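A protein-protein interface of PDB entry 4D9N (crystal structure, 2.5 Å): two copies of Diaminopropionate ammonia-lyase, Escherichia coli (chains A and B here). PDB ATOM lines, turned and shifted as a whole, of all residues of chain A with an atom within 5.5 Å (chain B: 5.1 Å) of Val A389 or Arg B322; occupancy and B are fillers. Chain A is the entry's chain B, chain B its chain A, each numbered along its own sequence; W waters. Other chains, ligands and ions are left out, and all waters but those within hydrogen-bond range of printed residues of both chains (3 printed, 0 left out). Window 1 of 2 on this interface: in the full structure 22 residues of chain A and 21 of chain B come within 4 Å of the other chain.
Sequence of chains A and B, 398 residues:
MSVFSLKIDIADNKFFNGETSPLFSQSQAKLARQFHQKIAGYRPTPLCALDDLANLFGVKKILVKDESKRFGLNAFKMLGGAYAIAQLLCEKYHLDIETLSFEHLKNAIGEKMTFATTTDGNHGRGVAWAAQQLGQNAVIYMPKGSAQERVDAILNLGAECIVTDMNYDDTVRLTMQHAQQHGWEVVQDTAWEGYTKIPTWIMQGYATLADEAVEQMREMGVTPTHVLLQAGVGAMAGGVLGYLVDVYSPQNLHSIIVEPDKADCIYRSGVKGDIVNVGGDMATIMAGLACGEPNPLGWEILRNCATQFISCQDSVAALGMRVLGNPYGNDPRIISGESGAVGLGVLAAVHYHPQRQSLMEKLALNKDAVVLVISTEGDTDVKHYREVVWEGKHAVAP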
ATOM      1  N   MET A 321      20.307   6.829 -15.455  1.00  0.00           N
ATOM      2  CA  MET A 321      19.398   7.294 -16.502  1.00  0.00           C
ATOM      3  C   MET A 321      19.610   8.778 -16.771  1.00  0.00           C
ATOM      4  O   MET A 321      19.795   9.187 -17.922  1.00  0.00           O
ATOM      5  CB  MET A 321      17.935   7.034 -16.116  1.00  0.00           C
ATOM      6  CG  MET A 321      17.517   5.572 -16.163  1.00  0.00           C
ATOM      7  SD  MET A 321      15.874   5.250 -15.490  1.00  0.00           S
ATOM      8  CE  MET A 321      14.814   5.830 -16.810  1.00  0.00           C
ATOM      9  N   ARG A 322      19.604   9.565 -15.694  1.00  0.00           N
ATOM     10  CA  ARG A 322      19.735  11.020 -15.765  1.00  0.00           C
ATOM     11  C   ARG A 322      21.109  11.477 -16.249  1.00  0.00           C
ATOM     12  O   ARG A 322      21.204  12.405 -17.060  1.00  0.00           O
ATOM     13  CB  ARG A 322      19.419  11.653 -14.410  1.00  0.00           C
ATOM     14  CG  ARG A 322      17.997  11.411 -13.935  1.00  0.00           C
ATOM     15  CD  ARG A 322      17.698  12.177 -12.662  1.00  0.00           C
ATOM     16  NE  ARG A 322      16.514  11.638 -12.009  1.00  0.00           N
ATOM     17  CZ  ARG A 322      16.534  10.807 -10.972  1.00  0.00           C
ATOM     18  NH1 ARG A 322      17.684  10.421 -10.436  1.00  0.00           N
ATOM     19  NH2 ARG A 322      15.394  10.369 -10.464  1.00  0.00           N
ATOM     20  N   ASN A 326      21.506  13.497 -19.678  1.00  0.00           N
ATOM     21  CA  ASN A 326      22.024  14.856 -19.594  1.00  0.00           C
ATOM     22  C   ASN A 326      23.518  14.807 -19.279  1.00  0.00           C
ATOM     23  O   ASN A 326      23.919  14.989 -18.128  1.00  0.00           O
ATOM     24  CB  ASN A 326      21.242  15.686 -18.567  1.00  0.00           C
ATOM     25  CG  ASN A 326      21.522  17.177 -18.674  1.00  0.00           C
ATOM     26  OD1 ASN A 326      22.486  17.606 -19.312  1.00  0.00           O
ATOM     27  ND2 ASN A 326      20.675  17.978 -18.034  1.00  0.00           N
ATOM     28  N   HIS A 384       7.767   6.043 -17.975  1.00  0.00           N
ATOM     29  CA  HIS A 384       8.683   5.875 -16.850  1.00  0.00           C
ATOM     30  C   HIS A 384       9.967   6.645 -17.026  1.00  0.00           C
ATOM     31  O   HIS A 384      10.476   7.228 -16.066  1.00  0.00           O
ATOM     32  CB  HIS A 384       8.972   4.394 -16.629  1.00  0.00           C
ATOM     33  CG  HIS A 384      10.018   4.125 -15.579  1.00  0.00           C
ATOM     34  ND1 HIS A 384       9.757   4.203 -14.263  1.00  0.00           N
ATOM     35  CD2 HIS A 384      11.362   3.777 -15.695  1.00  0.00           C
ATOM     36  CE1 HIS A 384      10.874   3.918 -13.567  1.00  0.00           C
ATOM     37  NE2 HIS A 384      11.855   3.657 -14.446  1.00  0.00           N
ATOM     38  N   TYR A 385      10.498   6.654 -18.249  1.00  0.00           N
ATOM     39  CA  TYR A 385      11.762   7.336 -18.547  1.00  0.00           C
ATOM     40  C   TYR A 385      11.699   8.840 -18.278  1.00  0.00           C
ATOM     41  O   TYR A 385      12.636   9.420 -17.725  1.00  0.00           O
ATOM     42  CB  TYR A 385      12.198   7.088 -19.997  1.00  0.00           C
ATOM     43  CG  TYR A 385      13.468   7.822 -20.372  1.00  0.00           C
ATOM     44  CD1 TYR A 385      14.718   7.275 -20.084  1.00  0.00           C
ATOM     45  CD2 TYR A 385      13.423   9.071 -20.998  1.00  0.00           C
ATOM     46  CE1 TYR A 385      15.884   7.946 -20.412  1.00  0.00           C
ATOM     47  CE2 TYR A 385      14.587   9.748 -21.329  1.00  0.00           C
ATOM     48  CZ  TYR A 385      15.813   9.180 -21.033  1.00  0.00           C
ATOM     49  OH  TYR A 385      16.975   9.837 -21.357  1.00  0.00           O
ATOM     50  N   ARG A 386      10.599   9.464 -18.685  1.00  0.00           N
ATOM     51  CA  ARG A 386      10.444  10.904 -18.537  1.00  0.00           C
ATOM     52  C   ARG A 386      10.072  11.292 -17.109  1.00  0.00           C
ATOM     53  O   ARG A 386      10.344  12.412 -16.678  1.00  0.00           O
ATOM     54  CB  ARG A 386       9.444  11.457 -19.555  1.00  0.00           C
ATOM     55  CG  ARG A 386       9.913  11.355 -21.004  1.00  0.00           C
ATOM     56  CD  ARG A 386      11.162  12.186 -21.276  1.00  0.00           C
ATOM     57  NE  ARG A 386      11.699  11.948 -22.617  1.00  0.00           N
ATOM     58  CZ  ARG A 386      12.781  12.543 -23.118  1.00  0.00           C
ATOM     59  NH1 ARG A 386      13.464  13.423 -22.394  1.00  0.00           N
ATOM     60  NH2 ARG A 386      13.182  12.258 -24.348  1.00  0.00           N
ATOM     61  N   GLU A 387       9.466  10.361 -16.376  1.00  0.00           N
ATOM     62  CA  GLU A 387       9.207  10.559 -14.951  1.00  0.00           C
ATOM     63  C   GLU A 387      10.515  10.603 -14.168  1.00  0.00           C
ATOM     64  O   GLU A 387      10.637  11.334 -13.184  1.00  0.00           O
ATOM     65  CB  GLU A 387       8.300   9.459 -14.405  1.00  0.00           C
ATOM     66  CG  GLU A 387       6.825   9.682 -14.694  1.00  0.00           C
ATOM     67  CD  GLU A 387       5.976   8.452 -14.446  1.00  0.00           C
ATOM     68  OE1 GLU A 387       6.517   7.428 -13.976  1.00  0.00           O
ATOM     69  OE2 GLU A 387       4.759   8.510 -14.726  1.00  0.00           O
ATOM     70  N   VAL A 388      11.491   9.820 -14.623  1.00  0.00           N
ATOM     71  CA  VAL A 388      12.797   9.760 -13.981  1.00  0.00           C
ATOM     72  C   VAL A 388      13.629  11.001 -14.302  1.00  0.00           C
ATOM     73  O   VAL A 388      14.106  11.682 -13.393  1.00  0.00           O
ATOM     74  CB  VAL A 388      13.561   8.472 -14.364  1.00  0.00           C
ATOM     75  CG1 VAL A 388      15.019   8.546 -13.924  1.00  0.00           C
ATOM     76  CG2 VAL A 388      12.882   7.251 -13.754  1.00  0.00           C
ATOM     77  N   VAL A 389      13.779  11.296 -15.593  1.00  0.00           N
ATOM     78  CA  VAL A 389      14.670  12.367 -16.045  1.00  0.00           C
ATOM     79  C   VAL A 389      14.072  13.773 -15.931  1.00  0.00           C
ATOM     80  O   VAL A 389      14.820  14.745 -15.831  1.00  0.00           O
ATOM     81  CB  VAL A 389      15.242  12.117 -17.468  1.00  0.00           C
ATOM     82  CG1 VAL A 389      15.918  10.754 -17.539  1.00  0.00           C
ATOM     83  CG2 VAL A 389      14.171  12.254 -18.544  1.00  0.00           C
ATOM     84  N   TRP A 390      12.741  13.880 -15.945  1.00  0.00           N
ATOM     85  CA  TRP A 390      12.070  15.183 -15.826  1.00  0.00           C
ATOM     86  C   TRP A 390      11.458  15.426 -14.476  1.00  0.00           C
ATOM     87  O   TRP A 390      11.694  16.470 -13.861  1.00  0.00           O
ATOM     88  CB  TRP A 390      11.000  15.362 -16.897  1.00  0.00           C
ATOM     89  CG  TRP A 390      11.515  15.527 -18.307  1.00  0.00           C
ATOM     90  CD1 TRP A 390      12.837  15.657 -18.726  1.00  0.00           C
ATOM     91  CD2 TRP A 390      10.716  15.634 -19.535  1.00  0.00           C
ATOM     92  NE1 TRP A 390      12.906  15.808 -20.087  1.00  0.00           N
ATOM     93  CE2 TRP A 390      11.673  15.806 -20.633  1.00  0.00           C
ATOM     94  CE3 TRP A 390       9.356  15.599 -19.825  1.00  0.00           C
ATOM     95  CZ2 TRP A 390      11.263  15.931 -21.954  1.00  0.00           C
ATOM     96  CZ3 TRP A 390       8.955  15.725 -21.161  1.00  0.00           C
ATOM     97  CH2 TRP A 390       9.886  15.889 -22.197  1.00  0.00           C
ATOM     98  N   GLU A 391      10.652  14.477 -14.008  1.00  0.00           N
ATOM     99  CA  GLU A 391       9.899  14.649 -12.765  1.00  0.00           C
ATOM    100  C   GLU A 391      10.757  14.339 -11.538  1.00  0.00           C
ATOM    101  O   GLU A 391      10.403  14.699 -10.410  1.00  0.00           O
ATOM    102  CB  GLU A 391       8.628  13.791 -12.772  1.00  0.00           C
ATOM    103  CG  GLU A 391       7.706  14.040 -13.958  1.00  0.00           C
ATOM    104  CD  GLU A 391       6.445  13.189 -13.929  1.00  0.00           C
ATOM    105  OE1 GLU A 391       6.050  12.726 -12.837  1.00  0.00           O
ATOM    106  OE2 GLU A 391       5.839  12.990 -15.002  1.00  0.00           O
ATOM    107  N   GLY A 392      11.888  13.678 -11.770  1.00  0.00           N
ATOM    108  CA  GLY A 392      12.800  13.296 -10.700  1.00  0.00           C
ATOM    109  C   GLY A 392      12.286  12.149  -9.850  1.00  0.00           C
ATOM    110  O   GLY A 392      12.565  12.094  -8.649  1.00  0.00           O
ATOM    111  N   ALA B 318      13.035  23.860 -11.445  1.00  0.00           N
ATOM    112  CA  ALA B 318      13.771  22.595 -11.510  1.00  0.00           C
ATOM    113  C   ALA B 318      13.242  21.677 -12.613  1.00  0.00           C
ATOM    114  O   ALA B 318      14.018  21.013 -13.303  1.00  0.00           O
ATOM    115  CB  ALA B 318      13.731  21.888 -10.162  1.00  0.00           C
ATOM    116  N   LEU B 319      11.918  21.649 -12.770  1.00  0.00           N
ATOM    117  CA  LEU B 319      11.272  20.885 -13.840  1.00  0.00           C
ATOM    118  C   LEU B 319      11.730  21.368 -15.217  1.00  0.00           C
ATOM    119  O   LEU B 319      12.036  20.554 -16.090  1.00  0.00           O
ATOM    120  CB  LEU B 319       9.746  20.966 -13.710  1.00  0.00           C
ATOM    121  CG  LEU B 319       8.853  20.362 -14.800  1.00  0.00           C
ATOM    122  CD1 LEU B 319       9.003  18.847 -14.884  1.00  0.00           C
ATOM    123  CD2 LEU B 319       7.403  20.746 -14.547  1.00  0.00           C
ATOM    124  N   GLY B 320      11.786  22.689 -15.391  1.00  0.00           N
ATOM    125  CA  GLY B 320      12.254  23.302 -16.636  1.00  0.00           C
ATOM    126  C   GLY B 320      13.693  22.953 -16.977  1.00  0.00           C
ATOM    127  O   GLY B 320      14.019  22.688 -18.137  1.00  0.00           O
ATOM    128  N   MET B 321      14.550  22.955 -15.956  1.00  0.00           N
ATOM    129  CA  MET B 321      15.960  22.614 -16.107  1.00  0.00           C
ATOM    130  C   MET B 321      16.107  21.227 -16.720  1.00  0.00           C
ATOM    131  O   MET B 321      16.890  21.028 -17.650  1.00  0.00           O
ATOM    132  CB  MET B 321      16.673  22.657 -14.751  1.00  0.00           C
ATOM    133  CG  MET B 321      16.762  24.039 -14.116  1.00  0.00           C
ATOM    134  SD  MET B 321      17.339  23.996 -12.406  1.00  0.00           S
ATOM    135  CE  MET B 321      19.074  23.621 -12.626  1.00  0.00           C
ATOM    136  N   ARG B 322      15.330  20.281 -16.203  1.00  0.00           N
ATOM    137  CA  ARG B 322      15.417  18.891 -16.620  1.00  0.00           C
ATOM    138  C   ARG B 322      14.870  18.674 -18.027  1.00  0.00           C
ATOM    139  O   ARG B 322      15.455  17.926 -18.812  1.00  0.00           O
ATOM    140  CB  ARG B 322      14.717  17.985 -15.607  1.00  0.00           C
ATOM    141  CG  ARG B 322      15.351  18.020 -14.225  1.00  0.00           C
ATOM    142  CD  ARG B 322      14.843  16.899 -13.337  1.00  0.00           C
ATOM    143  NE  ARG B 322      14.949  17.243 -11.923  1.00  0.00           N
ATOM    144  CZ  ARG B 322      13.947  17.719 -11.190  1.00  0.00           C
ATOM    145  NH1 ARG B 322      12.749  17.902 -11.729  1.00  0.00           N
ATOM    146  NH2 ARG B 322      14.140  18.008  -9.914  1.00  0.00           N
ATOM    147  N   VAL B 323      13.760  19.337 -18.343  1.00  0.00           N
ATOM    148  CA  VAL B 323      13.137  19.221 -19.664  1.00  0.00           C
ATOM    149  C   VAL B 323      14.061  19.780 -20.748  1.00  0.00           C
ATOM    150  O   VAL B 323      14.191  19.186 -21.820  1.00  0.00           O
ATOM    151  CB  VAL B 323      11.745  19.899 -19.716  1.00  0.00           C
ATOM    152  CG1 VAL B 323      11.178  19.868 -21.127  1.00  0.00           C
ATOM    153  CG2 VAL B 323      10.777  19.209 -18.764  1.00  0.00           C
ATOM    154  N   LEU B 324      14.706  20.909 -20.454  1.00  0.00           N
ATOM    155  CA  LEU B 324      15.645  21.535 -21.386  1.00  0.00           C
ATOM    156  C   LEU B 324      16.949  20.742 -21.518  1.00  0.00           C
ATOM    157  O   LEU B 324      17.487  20.601 -22.618  1.00  0.00           O
ATOM    158  CB  LEU B 324      15.934  22.985 -20.978  1.00  0.00           C
ATOM    159  CG  LEU B 324      14.841  24.023 -21.273  1.00  0.00           C
ATOM    160  CD1 LEU B 324      15.053  25.298 -20.471  1.00  0.00           C
ATOM    161  CD2 LEU B 324      14.734  24.341 -22.761  1.00  0.00           C
ATOM    162  N   GLY B 325      17.438  20.226 -20.390  1.00  0.00           N
ATOM    163  CA  GLY B 325      18.679  19.454 -20.343  1.00  0.00           C
ATOM    164  C   GLY B 325      18.572  18.056 -20.926  1.00  0.00           C
ATOM    165  O   GLY B 325      19.563  17.494 -21.385  1.00  0.00           O
ATOM    166  N   ASN B 326      17.370  17.488 -20.891  1.00  0.00           N
ATOM    167  CA  ASN B 326      17.094  16.218 -21.556  1.00  0.00           C
ATOM    168  C   ASN B 326      15.859  16.370 -22.438  1.00  0.00           C
ATOM    169  O   ASN B 326      14.751  16.040 -22.019  1.00  0.00           O
ATOM    170  CB  ASN B 326      16.911  15.089 -20.534  1.00  0.00           C
ATOM    171  CG  ASN B 326      17.078  13.704 -21.144  1.00  0.00           C
ATOM    172  OD1 ASN B 326      16.889  13.499 -22.347  1.00  0.00           O
ATOM    173  ND2 ASN B 326      17.427  12.740 -20.304  1.00  0.00           N
ATOM    174  N   PRO B 327      16.053  16.873 -23.670  1.00  0.00           N
ATOM    175  CA  PRO B 327      14.939  17.228 -24.549  1.00  0.00           C
ATOM    176  C   PRO B 327      14.150  16.020 -25.052  1.00  0.00           C
ATOM    177  O   PRO B 327      14.646  14.891 -25.031  1.00  0.00           O
ATOM    178  CB  PRO B 327      15.627  17.950 -25.713  1.00  0.00           C
ATOM    179  CG  PRO B 327      17.003  17.380 -25.745  1.00  0.00           C
ATOM    180  CD  PRO B 327      17.361  17.096 -24.315  1.00  0.00           C
ATOM    181  N   VAL B 388      20.112  19.052  -9.482  1.00  0.00           N
ATOM    182  CA  VAL B 388      18.763  19.072 -10.044  1.00  0.00           C
ATOM    183  C   VAL B 388      18.599  18.026 -11.149  1.00  0.00           C
ATOM    184  O   VAL B 388      17.689  17.198 -11.084  1.00  0.00           O
ATOM    185  CB  VAL B 388      18.361  20.484 -10.544  1.00  0.00           C
ATOM    186  CG1 VAL B 388      17.084  20.432 -11.371  1.00  0.00           C
ATOM    187  CG2 VAL B 388      18.187  21.438  -9.368  1.00  0.00           C
ATOM    188  N   VAL B 389      19.486  18.050 -12.145  1.00  0.00           N
ATOM    189  CA  VAL B 389      19.326  17.192 -13.332  1.00  0.00           C
ATOM    190  C   VAL B 389      19.753  15.730 -13.158  1.00  0.00           C
ATOM    191  O   VAL B 389      19.214  14.855 -13.834  1.00  0.00           O
ATOM    192  CB  VAL B 389      19.962  17.791 -14.617  1.00  0.00           C
ATOM    193  CG1 VAL B 389      19.365  19.161 -14.921  1.00  0.00           C
ATOM    194  CG2 VAL B 389      21.484  17.850 -14.528  1.00  0.00           C
ATOM    195  N   GLY B 392      18.031  14.691  -8.937  1.00  0.00           N
ATOM    196  CA  GLY B 392      16.588  14.863  -8.841  1.00  0.00           C
ATOM    197  C   GLY B 392      16.188  15.721  -7.656  1.00  0.00           C
ATOM    198  O   GLY B 392      15.124  15.520  -7.065  1.00  0.00           O
ATOM    199  N   LYS B 393      17.052  16.672  -7.306  1.00  0.00           N
ATOM    200  CA  LYS B 393      16.768  17.637  -6.249  1.00  0.00           C
ATOM    201  C   LYS B 393      15.580  18.501  -6.658  1.00  0.00           C
ATOM    202  O   LYS B 393      15.405  18.806  -7.842  1.00  0.00           O
ATOM    203  CB  LYS B 393      17.995  18.512  -5.970  1.00  0.00           C
ATOM    204  CG  LYS B 393      18.042  19.105  -4.567  1.00  0.00           C
ATOM    205  CD  LYS B 393      19.325  19.890  -4.322  1.00  0.00           C
ATOM    206  CE  LYS B 393      19.312  21.235  -5.037  1.00  0.00           C
ATOM    207  NZ  LYS B 393      20.525  22.046  -4.738  1.00  0.00           N
ATOM    208  N   HIS B 394      14.769  18.882  -5.673  1.00  0.00           N
ATOM    209  CA  HIS B 394      13.522  19.615  -5.904  1.00  0.00           C
ATOM    210  C   HIS B 394      12.660  18.896  -6.903  1.00  0.00           C
ATOM    211  O   HIS B 394      12.272  19.457  -7.931  1.00  0.00           O
ATOM    212  CB  HIS B 394      13.791  21.059  -6.334  1.00  0.00           C
ATOM    213  CG  HIS B 394      14.635  21.836  -5.354  1.00  0.00           C
ATOM    214  ND1 HIS B 394      15.815  22.383  -5.693  1.00  0.00           N
ATOM    215  CD2 HIS B 394      14.434  22.135  -4.007  1.00  0.00           C
ATOM    216  CE1 HIS B 394      16.342  23.010  -4.623  1.00  0.00           C
ATOM    217  NE2 HIS B 394      15.497  22.853  -3.593  1.00  0.00           N
ATOM    218  N   ALA B 395      12.364  17.635  -6.598  1.00  0.00           N
ATOM    219  CA  ALA B 395      11.558  16.782  -7.463  1.00  0.00           C
ATOM    220  C   ALA B 395      10.077  17.154  -7.413  1.00  0.00           C
ATOM    221  O   ALA B 395       9.675  18.083  -6.710  1.00  0.00           O
ATOM    222  CB  ALA B 395      11.759  15.319  -7.092  1.00  0.00           C
HETATM  223  O   HOH W   1      18.006  17.098 -17.824  1.00  0.00           O
HETATM  224  O   HOH W   2      18.650  13.275 -17.868  1.00  0.00           O
HETATM  225  O   HOH W   3      17.528  15.033 -16.050  1.00  0.00           O
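The guanidinium group (NH1) of Arg B322 lies within hydrogen-bond range of the backbone carbonyl oxygen (O) of Trp A390 (2.8 Å). The guanidinium group (NH1) of Arg A386 sits at hydrogen-bond distance from the backbone carbonyl oxygen (O) of Asn B326, 2.9 Å away. The side-chain amide nitrogen (ND2) of Asn B326 sits at hydrogen-bond distance from the side-chain hydroxyl (OH) of Tyr A385. The backbone carbonyl oxygen (O) of Asn B326 sits at hydrogen-bond distance from the indole nitrogen (NE1) of Trp A390 (2.7 Å). The guanidinium group (NH2) of Arg A386 is in hydrogen-bond range of the backbone carbonyl oxygen (O) of Pro B327 (3.1 Å).
Of the 12 printed residues of chain A, 8 touch a printed residue of chain B. Hydrophobic or aromatic side chains of chain B within 4 Å of the printed part of chain A: Leu B319, Val B323, Val B389 and Ala B395.
O of Glu A387 sits at hydrogen-bond distance from N of Gly A392 (3.0 Å). NH2 of Arg B322 sits at hydrogen-bond distance from O of Lys B393, 2.6 Å away. The guanidinium group of Arg B322 sits at hydrogen-bond distance from the backbone carbonyl oxygen of His B394 (3.1 Å). O of Arg A386 sits at hydrogen-bond distance from N of Glu A391 (3.4 Å). NE of Arg A322 lies within hydrogen-bond range of O of Val A388. The backbone carbonyl oxygen (O) of Val B388 sits at hydrogen-bond distance from the guanidinium group (NE) of Arg B322 (2.9 Å).
Arg A322 touches Val B389, and with the chains exchanged Val A389 touches Arg B322. Asn A326 touches Val B389, and with the chains exchanged Val A389 touches Asn B326. Of the 14 pairs that touch across the chains among the printed residues, 4 have their exchanged pair printed and touching as well.
Among the printed residues, merely in contact across the chains: Val A389 with Arg B322 (3.2 Å), Arg A322 with Val B389 (3.3 Å), Asn A326 with Gly B325 (3.4 Å), Trp A390 with Val B323 (3.4 Å), Asn A326 with Val B389 (3.5 Å), Val A389 with Asn B326 (3.6 Å), Glu A391 with Ala B395 (3.6 Å), Gly A392 with Ala B395 (3.7 Å) and Trp A390 with Leu B319 (3.7 Å).
Met A321 touches none of the printed residues of chain B. Glu A387 touches none of the printed residues of chain B. Of chain B, only Arg B322 and Asn B326 come within 4 Å of Val A389. Printed residues of chain B within 4 Å of Trp A390: Leu B319 (3.7 Å), Arg B322 (2.8 Å), Val B323 (3.4 Å) and Asn B326 (2.7 Å). Arg B322 touches just these residues of chain A: Val A389 (3.2 Å) and Trp A390 (2.8 Å). Printed residues of chain A within 4 Å of Val B323: Trp A390 (3.4 Å). Of the printed residues of chain A, Gly B325 touches Asn A326.
Water W3 lies within hydrogen-bond range of the backbone carbonyl oxygen of Val A389 (2.7 Å) and the backbone carbonyl oxygen of Val B389 (2.8 Å). Water W2 lies within hydrogen-bond range of ND2 of Asn B326 (2.8 Å), O of Arg A322 (2.8 Å) and N of Asn A326 (3.4 Å). Water W1 lies within hydrogen-bond range of ND2 of Asn A326 (2.8 Å), O of Arg B322 (2.9 Å) and N of Asn B326 (3.2 Å).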
